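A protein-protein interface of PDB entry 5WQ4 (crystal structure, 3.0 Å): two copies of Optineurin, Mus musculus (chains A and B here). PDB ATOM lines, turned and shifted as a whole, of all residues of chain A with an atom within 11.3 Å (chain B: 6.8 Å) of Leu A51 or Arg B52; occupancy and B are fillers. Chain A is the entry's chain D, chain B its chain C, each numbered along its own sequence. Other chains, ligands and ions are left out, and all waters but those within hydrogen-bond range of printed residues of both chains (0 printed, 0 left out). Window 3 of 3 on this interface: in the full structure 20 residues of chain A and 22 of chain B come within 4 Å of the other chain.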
ATOM      1  N   GLU A  42       5.715  27.085  29.596  1.00  0.00           N
ATOM      2  CA  GLU A  42       6.633  28.105  30.109  1.00  0.00           C
ATOM      3  C   GLU A  42       7.950  27.459  30.547  1.00  0.00           C
ATOM      4  O   GLU A  42       9.032  28.061  30.419  1.00  0.00           O
ATOM      5  CB  GLU A  42       6.008  28.875  31.279  1.00  0.00           C
ATOM      6  N   GLU A  43       7.855  26.244  31.095  1.00  0.00           N
ATOM      7  CA  GLU A  43       9.070  25.505  31.448  1.00  0.00           C
ATOM      8  C   GLU A  43       9.896  25.203  30.188  1.00  0.00           C
ATOM      9  O   GLU A  43      11.116  25.383  30.165  1.00  0.00           O
ATOM     10  CB  GLU A  43       8.740  24.218  32.231  1.00  0.00           C
ATOM     11  CG  GLU A  43       8.758  22.921  31.444  1.00  0.00           C
ATOM     12  CD  GLU A  43       8.492  21.707  32.306  1.00  0.00           C
ATOM     13  OE1 GLU A  43       9.065  20.637  31.992  1.00  0.00           O
ATOM     14  OE2 GLU A  43       7.717  21.821  33.290  1.00  0.00           O
ATOM     15  N   ASP A  44       9.224  24.745  29.141  1.00  0.00           N
ATOM     16  CA  ASP A  44       9.885  24.449  27.879  1.00  0.00           C
ATOM     17  C   ASP A  44      10.473  25.723  27.264  1.00  0.00           C
ATOM     18  O   ASP A  44      11.492  25.683  26.584  1.00  0.00           O
ATOM     19  CB  ASP A  44       8.896  23.758  26.944  1.00  0.00           C
ATOM     20  CG  ASP A  44       8.597  22.330  27.379  1.00  0.00           C
ATOM     21  OD1 ASP A  44       9.108  21.913  28.442  1.00  0.00           O
ATOM     22  OD2 ASP A  44       7.813  21.641  26.698  1.00  0.00           O
ATOM     23  N   LEU A  45       9.822  26.853  27.508  1.00  0.00           N
ATOM     24  CA  LEU A  45      10.317  28.137  27.030  1.00  0.00           C
ATOM     25  C   LEU A  45      11.610  28.480  27.770  1.00  0.00           C
ATOM     26  O   LEU A  45      12.539  29.034  27.183  1.00  0.00           O
ATOM     27  CB  LEU A  45       9.258  29.235  27.221  1.00  0.00           C
ATOM     28  N   GLU A  46      11.664  28.163  29.062  1.00  0.00           N
ATOM     29  CA  GLU A  46      12.916  28.275  29.807  1.00  0.00           C
ATOM     30  C   GLU A  46      14.014  27.364  29.237  1.00  0.00           C
ATOM     31  O   GLU A  46      15.124  27.825  28.940  1.00  0.00           O
ATOM     32  CB  GLU A  46      12.694  27.942  31.290  1.00  0.00           C
ATOM     33  CG  GLU A  46      12.421  29.142  32.195  1.00  0.00           C
ATOM     34  CD  GLU A  46      13.586  29.457  33.119  1.00  0.00           C
ATOM     35  OE1 GLU A  46      13.889  28.629  34.005  1.00  0.00           O
ATOM     36  OE2 GLU A  46      14.205  30.531  32.952  1.00  0.00           O
ATOM     37  N   THR A  47      13.694  26.082  29.052  1.00  0.00           N
ATOM     38  CA  THR A  47      14.674  25.124  28.530  1.00  0.00           C
ATOM     39  C   THR A  47      15.258  25.564  27.193  1.00  0.00           C
ATOM     40  O   THR A  47      16.477  25.590  27.006  1.00  0.00           O
ATOM     41  CB  THR A  47      14.056  23.718  28.365  1.00  0.00           C
ATOM     42  OG1 THR A  47      13.842  23.134  29.658  1.00  0.00           O
ATOM     43  CG2 THR A  47      14.985  22.822  27.585  1.00  0.00           C
ATOM     44  N   MET A  48      14.376  25.938  26.276  1.00  0.00           N
ATOM     45  CA  MET A  48      14.781  26.394  24.956  1.00  0.00           C
ATOM     46  C   MET A  48      15.572  27.709  25.070  1.00  0.00           C
ATOM     47  O   MET A  48      16.469  27.987  24.253  1.00  0.00           O
ATOM     48  CB  MET A  48      13.564  26.538  24.058  1.00  0.00           C
ATOM     49  CG  MET A  48      13.850  27.145  22.711  1.00  0.00           C
ATOM     50  SD  MET A  48      12.350  27.769  21.920  1.00  0.00           S
ATOM     51  CE  MET A  48      12.902  29.383  21.366  1.00  0.00           C
ATOM     52  N   ALA A  49      15.237  28.516  26.078  1.00  0.00           N
ATOM     53  CA  ALA A  49      16.007  29.726  26.347  1.00  0.00           C
ATOM     54  C   ALA A  49      17.448  29.324  26.642  1.00  0.00           C
ATOM     55  O   ALA A  49      18.377  30.007  26.210  1.00  0.00           O
ATOM     56  CB  ALA A  49      15.414  30.522  27.495  1.00  0.00           C
ATOM     57  N   VAL A  50      17.641  28.253  27.416  1.00  0.00           N
ATOM     58  CA  VAL A  50      19.010  27.757  27.627  1.00  0.00           C
ATOM     59  C   VAL A  50      19.637  27.183  26.340  1.00  0.00           C
ATOM     60  O   VAL A  50      20.822  27.387  26.081  1.00  0.00           O
ATOM     61  CB  VAL A  50      19.098  26.672  28.775  1.00  0.00           C
ATOM     62  CG1 VAL A  50      17.838  26.625  29.611  1.00  0.00           C
ATOM     63  CG2 VAL A  50      19.480  25.276  28.246  1.00  0.00           C
ATOM     64  N   LEU A  51      18.840  26.487  25.537  1.00  0.00           N
ATOM     65  CA  LEU A  51      19.342  25.859  24.329  1.00  0.00           C
ATOM     66  C   LEU A  51      19.888  26.892  23.341  1.00  0.00           C
ATOM     67  O   LEU A  51      20.859  26.616  22.636  1.00  0.00           O
ATOM     68  CB  LEU A  51      18.254  24.997  23.677  1.00  0.00           C
ATOM     69  CG  LEU A  51      18.654  23.810  22.785  1.00  0.00           C
ATOM     70  CD1 LEU A  51      20.131  23.477  22.926  1.00  0.00           C
ATOM     71  CD2 LEU A  51      17.816  22.562  23.088  1.00  0.00           C
ATOM     72  N   ARG A  52      19.264  28.062  23.253  1.00  0.00           N
ATOM     73  CA  ARG A  52      19.760  29.079  22.313  1.00  0.00           C
ATOM     74  C   ARG A  52      21.114  29.619  22.800  1.00  0.00           C
ATOM     75  O   ARG A  52      22.039  29.840  22.012  1.00  0.00           O
ATOM     76  CB  ARG A  52      18.737  30.216  22.113  1.00  0.00           C
ATOM     77  N   ALA A  53      21.211  29.875  24.098  1.00  0.00           N
ATOM     78  CA  ALA A  53      22.474  30.290  24.697  1.00  0.00           C
ATOM     79  C   ALA A  53      23.545  29.258  24.376  1.00  0.00           C
ATOM     80  O   ALA A  53      24.656  29.602  23.957  1.00  0.00           O
ATOM     81  CB  ALA A  53      22.325  30.461  26.199  1.00  0.00           C
ATOM     82  N   GLN A  54      23.185  27.986  24.549  1.00  0.00           N
ATOM     83  CA  GLN A  54      24.096  26.883  24.273  1.00  0.00           C
ATOM     84  C   GLN A  54      24.569  26.894  22.831  1.00  0.00           C
ATOM     85  O   GLN A  54      25.768  26.784  22.581  1.00  0.00           O
ATOM     86  CB  GLN A  54      23.462  25.524  24.589  1.00  0.00           C
ATOM     87  CG  GLN A  54      24.510  24.410  24.683  1.00  0.00           C
ATOM     88  CD  GLN A  54      23.989  23.110  25.267  1.00  0.00           C
ATOM     89  OE1 GLN A  54      22.788  22.940  25.487  1.00  0.00           O
ATOM     90  NE2 GLN A  54      24.907  22.196  25.564  1.00  0.00           N
ATOM     91  N   MET A  55      23.638  27.029  21.891  1.00  0.00           N
ATOM     92  CA  MET A  55      24.001  27.006  20.486  1.00  0.00           C
ATOM     93  C   MET A  55      24.886  28.181  20.111  1.00  0.00           C
ATOM     94  O   MET A  55      25.820  28.031  19.311  1.00  0.00           O
ATOM     95  CB  MET A  55      22.749  26.996  19.619  1.00  0.00           C
ATOM     96  CG  MET A  55      22.968  27.462  18.188  1.00  0.00           C
ATOM     97  SD  MET A  55      22.481  29.183  17.908  1.00  0.00           S
ATOM     98  CE  MET A  55      23.672  29.707  16.669  1.00  0.00           C
ATOM     99  N   GLU A  56      24.620  29.350  20.691  1.00  0.00           N
ATOM    100  CA  GLU A  56      25.480  30.493  20.391  1.00  0.00           C
ATOM    101  C   GLU A  56      26.882  30.290  20.968  1.00  0.00           C
ATOM    102  O   GLU A  56      27.868  30.644  20.323  1.00  0.00           O
ATOM    103  CB  GLU A  56      24.857  31.818  20.853  1.00  0.00           C
ATOM    104  CG  GLU A  56      23.710  32.269  19.944  1.00  0.00           C
ATOM    105  CD  GLU A  56      23.245  33.700  20.192  1.00  0.00           C
ATOM    106  OE1 GLU A  56      23.821  34.387  21.061  1.00  0.00           O
ATOM    107  OE2 GLU A  56      22.301  34.148  19.502  1.00  0.00           O
ATOM    108  N   VAL A  57      26.974  29.705  22.161  1.00  0.00           N
ATOM    109  CA  VAL A  57      28.287  29.360  22.734  1.00  0.00           C
ATOM    110  C   VAL A  57      29.050  28.248  21.959  1.00  0.00           C
ATOM    111  O   VAL A  57      30.249  28.378  21.700  1.00  0.00           O
ATOM    112  CB  VAL A  57      28.155  28.963  24.212  1.00  0.00           C
ATOM    113  CG1 VAL A  57      29.438  28.342  24.708  1.00  0.00           C
ATOM    114  CG2 VAL A  57      27.834  30.191  25.046  1.00  0.00           C
ATOM    115  N   TYR A  58      28.380  27.153  21.610  1.00  0.00           N
ATOM    116  CA  TYR A  58      29.048  26.100  20.851  1.00  0.00           C
ATOM    117  C   TYR A  58      29.512  26.609  19.510  1.00  0.00           C
ATOM    118  O   TYR A  58      30.546  26.171  19.007  1.00  0.00           O
ATOM    119  CB  TYR A  58      28.163  24.874  20.632  1.00  0.00           C
ATOM    120  CG  TYR A  58      27.943  24.092  21.894  1.00  0.00           C
ATOM    121  CD1 TYR A  58      28.597  24.445  23.063  1.00  0.00           C
ATOM    122  CD2 TYR A  58      27.172  22.948  21.896  1.00  0.00           C
ATOM    123  CE1 TYR A  58      28.424  23.735  24.206  1.00  0.00           C
ATOM    124  CE2 TYR A  58      27.001  22.223  23.037  1.00  0.00           C
ATOM    125  CZ  TYR A  58      27.629  22.621  24.188  1.00  0.00           C
ATOM    126  OH  TYR A  58      27.455  21.905  25.337  1.00  0.00           O
ATOM    127  N   CYS A  59      28.716  27.489  18.915  1.00  0.00           N
ATOM    128  CA  CYS A  59      29.090  28.135  17.666  1.00  0.00           C
ATOM    129  C   CYS A  59      30.347  29.025  17.856  1.00  0.00           C
ATOM    130  O   CYS A  59      31.297  29.002  17.055  1.00  0.00           O
ATOM    131  CB  CYS A  59      27.898  28.936  17.129  1.00  0.00           C
ATOM    132  SG  CYS A  59      28.112  29.559  15.456  1.00  0.00           S
ATOM    133  N   SER A  60      30.328  29.832  18.911  1.00  0.00           N
ATOM    134  CA  SER A  60      31.462  30.693  19.233  1.00  0.00           C
ATOM    135  C   SER A  60      32.765  29.872  19.405  1.00  0.00           C
ATOM    136  O   SER A  60      33.822  30.216  18.855  1.00  0.00           O
ATOM    137  CB  SER A  60      31.142  31.503  20.502  1.00  0.00           C
ATOM    138  OG  SER A  60      31.765  32.778  20.505  1.00  0.00           O
ATOM    139  N   THR B  47      10.530  25.806  17.015  1.00  0.00           N
ATOM    140  CA  THR B  47      11.785  26.524  16.916  1.00  0.00           C
ATOM    141  C   THR B  47      12.807  25.751  17.742  1.00  0.00           C
ATOM    142  O   THR B  47      13.915  25.473  17.266  1.00  0.00           O
ATOM    143  CB  THR B  47      11.668  27.992  17.385  1.00  0.00           C
ATOM    144  N   MET B  48      12.413  25.307  18.934  1.00  0.00           N
ATOM    145  CA  MET B  48      13.382  24.621  19.801  1.00  0.00           C
ATOM    146  C   MET B  48      13.951  23.318  19.239  1.00  0.00           C
ATOM    147  O   MET B  48      15.148  23.044  19.422  1.00  0.00           O
ATOM    148  CB  MET B  48      12.759  24.300  21.157  1.00  0.00           C
ATOM    149  CG  MET B  48      13.684  23.525  22.087  1.00  0.00           C
ATOM    150  SD  MET B  48      12.780  22.668  23.390  1.00  0.00           S
ATOM    151  CE  MET B  48      12.268  21.179  22.515  1.00  0.00           C
ATOM    152  N   ALA B  49      13.137  22.533  18.534  1.00  0.00           N
ATOM    153  CA  ALA B  49      13.724  21.312  17.943  1.00  0.00           C
ATOM    154  C   ALA B  49      14.853  21.600  16.930  1.00  0.00           C
ATOM    155  O   ALA B  49      15.975  21.006  17.003  1.00  0.00           O
ATOM    156  CB  ALA B  49      12.643  20.460  17.281  1.00  0.00           C
ATOM    157  N   VAL B  50      14.605  22.539  16.013  1.00  0.00           N
ATOM    158  CA  VAL B  50      15.723  22.827  15.084  1.00  0.00           C
ATOM    159  C   VAL B  50      16.896  23.417  15.900  1.00  0.00           C
ATOM    160  O   VAL B  50      18.071  23.174  15.583  1.00  0.00           O
ATOM    161  CB  VAL B  50      15.344  23.757  13.896  1.00  0.00           C
ATOM    162  N   LEU B  51      16.585  24.168  16.956  1.00  0.00           N
ATOM    163  CA  LEU B  51      17.640  24.760  17.779  1.00  0.00           C
ATOM    164  C   LEU B  51      18.592  23.693  18.386  1.00  0.00           C
ATOM    165  O   LEU B  51      19.820  23.888  18.443  1.00  0.00           O
ATOM    166  CB  LEU B  51      17.012  25.612  18.899  1.00  0.00           C
ATOM    167  N   ARG B  52      18.031  22.560  18.813  1.00  0.00           N
ATOM    168  CA  ARG B  52      18.834  21.500  19.413  1.00  0.00           C
ATOM    169  C   ARG B  52      19.724  20.882  18.351  1.00  0.00           C
ATOM    170  O   ARG B  52      20.968  20.729  18.548  1.00  0.00           O
ATOM    171  CB  ARG B  52      17.949  20.424  20.048  1.00  0.00           C
ATOM    172  CG  ARG B  52      18.706  19.472  20.979  1.00  0.00           C
ATOM    173  CD  ARG B  52      17.771  18.632  21.845  1.00  0.00           C
ATOM    174  N   ALA B  53      19.103  20.586  17.200  1.00  0.00           N
ATOM    175  CA  ALA B  53      19.889  20.023  16.090  1.00  0.00           C
ATOM    176  C   ALA B  53      21.114  20.898  15.789  1.00  0.00           C
ATOM    177  O   ALA B  53      22.250  20.427  15.638  1.00  0.00           O
ATOM    178  CB  ALA B  53      19.032  19.881  14.855  1.00  0.00           C
ATOM    179  N   GLN B  54      20.871  22.194  15.743  1.00  0.00           N
ATOM    180  CA  GLN B  54      21.920  23.149  15.449  1.00  0.00           C
ATOM    181  C   GLN B  54      23.093  23.067  16.435  1.00  0.00           C
ATOM    182  O   GLN B  54      24.259  22.981  16.009  1.00  0.00           O
ATOM    183  CB  GLN B  54      21.337  24.565  15.451  1.00  0.00           C
ATOM    184  CG  GLN B  54      22.200  25.570  14.787  1.00  0.00           C
ATOM    185  CD  GLN B  54      21.507  26.868  14.660  1.00  0.00           C
ATOM    186  OE1 GLN B  54      20.421  27.040  15.192  1.00  0.00           O
ATOM    187  NE2 GLN B  54      22.132  27.816  13.981  1.00  0.00           N
ATOM    188  N   MET B  55      22.807  23.078  17.743  1.00  0.00           N
ATOM    189  CA  MET B  55      23.926  23.068  18.693  1.00  0.00           C
ATOM    190  C   MET B  55      24.703  21.744  18.604  1.00  0.00           C
ATOM    191  O   MET B  55      25.931  21.711  18.762  1.00  0.00           O
ATOM    192  CB  MET B  55      23.452  23.351  20.120  1.00  0.00           C
ATOM    193  CG  MET B  55      22.726  22.220  20.786  1.00  0.00           C
ATOM    194  SD  MET B  55      23.792  21.157  21.771  1.00  0.00           S
ATOM    195  CE  MET B  55      22.612  19.885  22.262  1.00  0.00           C
ATOM    196  N   GLU B  56      24.000  20.658  18.310  1.00  0.00           N
ATOM    197  CA  GLU B  56      24.667  19.369  18.179  1.00  0.00           C
ATOM    198  C   GLU B  56      25.657  19.436  17.028  1.00  0.00           C
ATOM    199  O   GLU B  56      26.782  18.934  17.111  1.00  0.00           O
ATOM    200  CB  GLU B  56      23.621  18.298  17.942  1.00  0.00           C
ATOM    201  CG  GLU B  56      22.794  18.088  19.187  1.00  0.00           C
ATOM    202  CD  GLU B  56      21.754  17.018  19.049  1.00  0.00           C
ATOM    203  OE1 GLU B  56      21.660  16.404  17.961  1.00  0.00           O
ATOM    204  OE2 GLU B  56      21.002  16.834  20.032  1.00  0.00           O
ATOM    205  N   VAL B  57      25.261  20.122  15.965  1.00  0.00           N
ATOM    206  CA  VAL B  57      26.184  20.328  14.851  1.00  0.00           C
ATOM    207  C   VAL B  57      27.400  21.126  15.271  1.00  0.00           C
ATOM    208  O   VAL B  57      28.518  20.710  15.013  1.00  0.00           O
ATOM    209  CB  VAL B  57      25.519  21.063  13.665  1.00  0.00           C
ATOM    210  CG1 VAL B  57      26.564  21.628  12.741  1.00  0.00           C
ATOM    211  CG2 VAL B  57      24.566  20.153  12.925  1.00  0.00           C
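Met A48 touches its own counterpart, Met B48. Leu A51 touches Arg B52, but with the chains exchanged Arg A52 does not touch Leu B51 (5.5 Å). Leu A51 touches Met B55, but with the chains exchanged Met A55 does not touch Leu B51 (4.4 Å). Met A55 touches Gln B54, but with the chains exchanged Gln A54 does not touch Met B55 (4.01 Å). 11 positions are printed for both chains.
Among the printed residues, pairs that only touch across the chains: Met A48 with Met B48 (3.4 Å), Leu A51 with Arg B52 (3.7 Å), Leu A51 with Met B55 (3.6 Å), Met A55 with Gln B54 (3.6 Å), Met A55 with Met B55 (3.7 Å) and Tyr A58 with Met B55 (3.6 Å).
Of the 11 printed residues of chain B, 4 touch a printed residue of chain A. Hydrophobic or aromatic side chains of chain A within 4 Å of the printed part of chain B: Met A48, Leu A51, Met A55 and Tyr A58. Among the printed residues, no Asp or Glu carboxylate lies within 4 Å of a Lys or Arg side-chain nitrogen of the other chain.
Leu A51 touches just these residues of chain B: Arg B52 (3.7 Å) and Met B55 (3.6 Å). Arg B52 touches just one residue of chain A: Leu A51 (3.7 Å). Met B48 touches just one residue of chain A: Met A48. Ala B49 touches none of the printed residues of chain A. No residue of chain A comes within 4 Å of Val B50. No residue of chain A comes within 4 Å of Leu B51. No residue of chain A comes within 4 Å of Ala B53. Of the printed residues of chain A, Gln B54 touches Met A55. Of the printed residues of chain B, Tyr A58 touches Met B55 (3.6 Å). Printed residues of chain A within 4 Å of Met B55: Leu A51 (3.6 Å), Met A55 (3.7 Å) and Tyr A58 (3.6 Å). Val A50 touches none of the printed residues of chain B. The nearest residue of chain B that does not touch Leu A51 is Met B48 (4.4 Å). The nearest printed residue of chain A that does not touch Gln B54 is Tyr A58 (6.3 Å).
The side-chain amide nitrogen (NE2) of Gln A54 sits at hydrogen-bond distance from the side-chain hydroxyl (OH) of Tyr A58 (2.6 Å).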
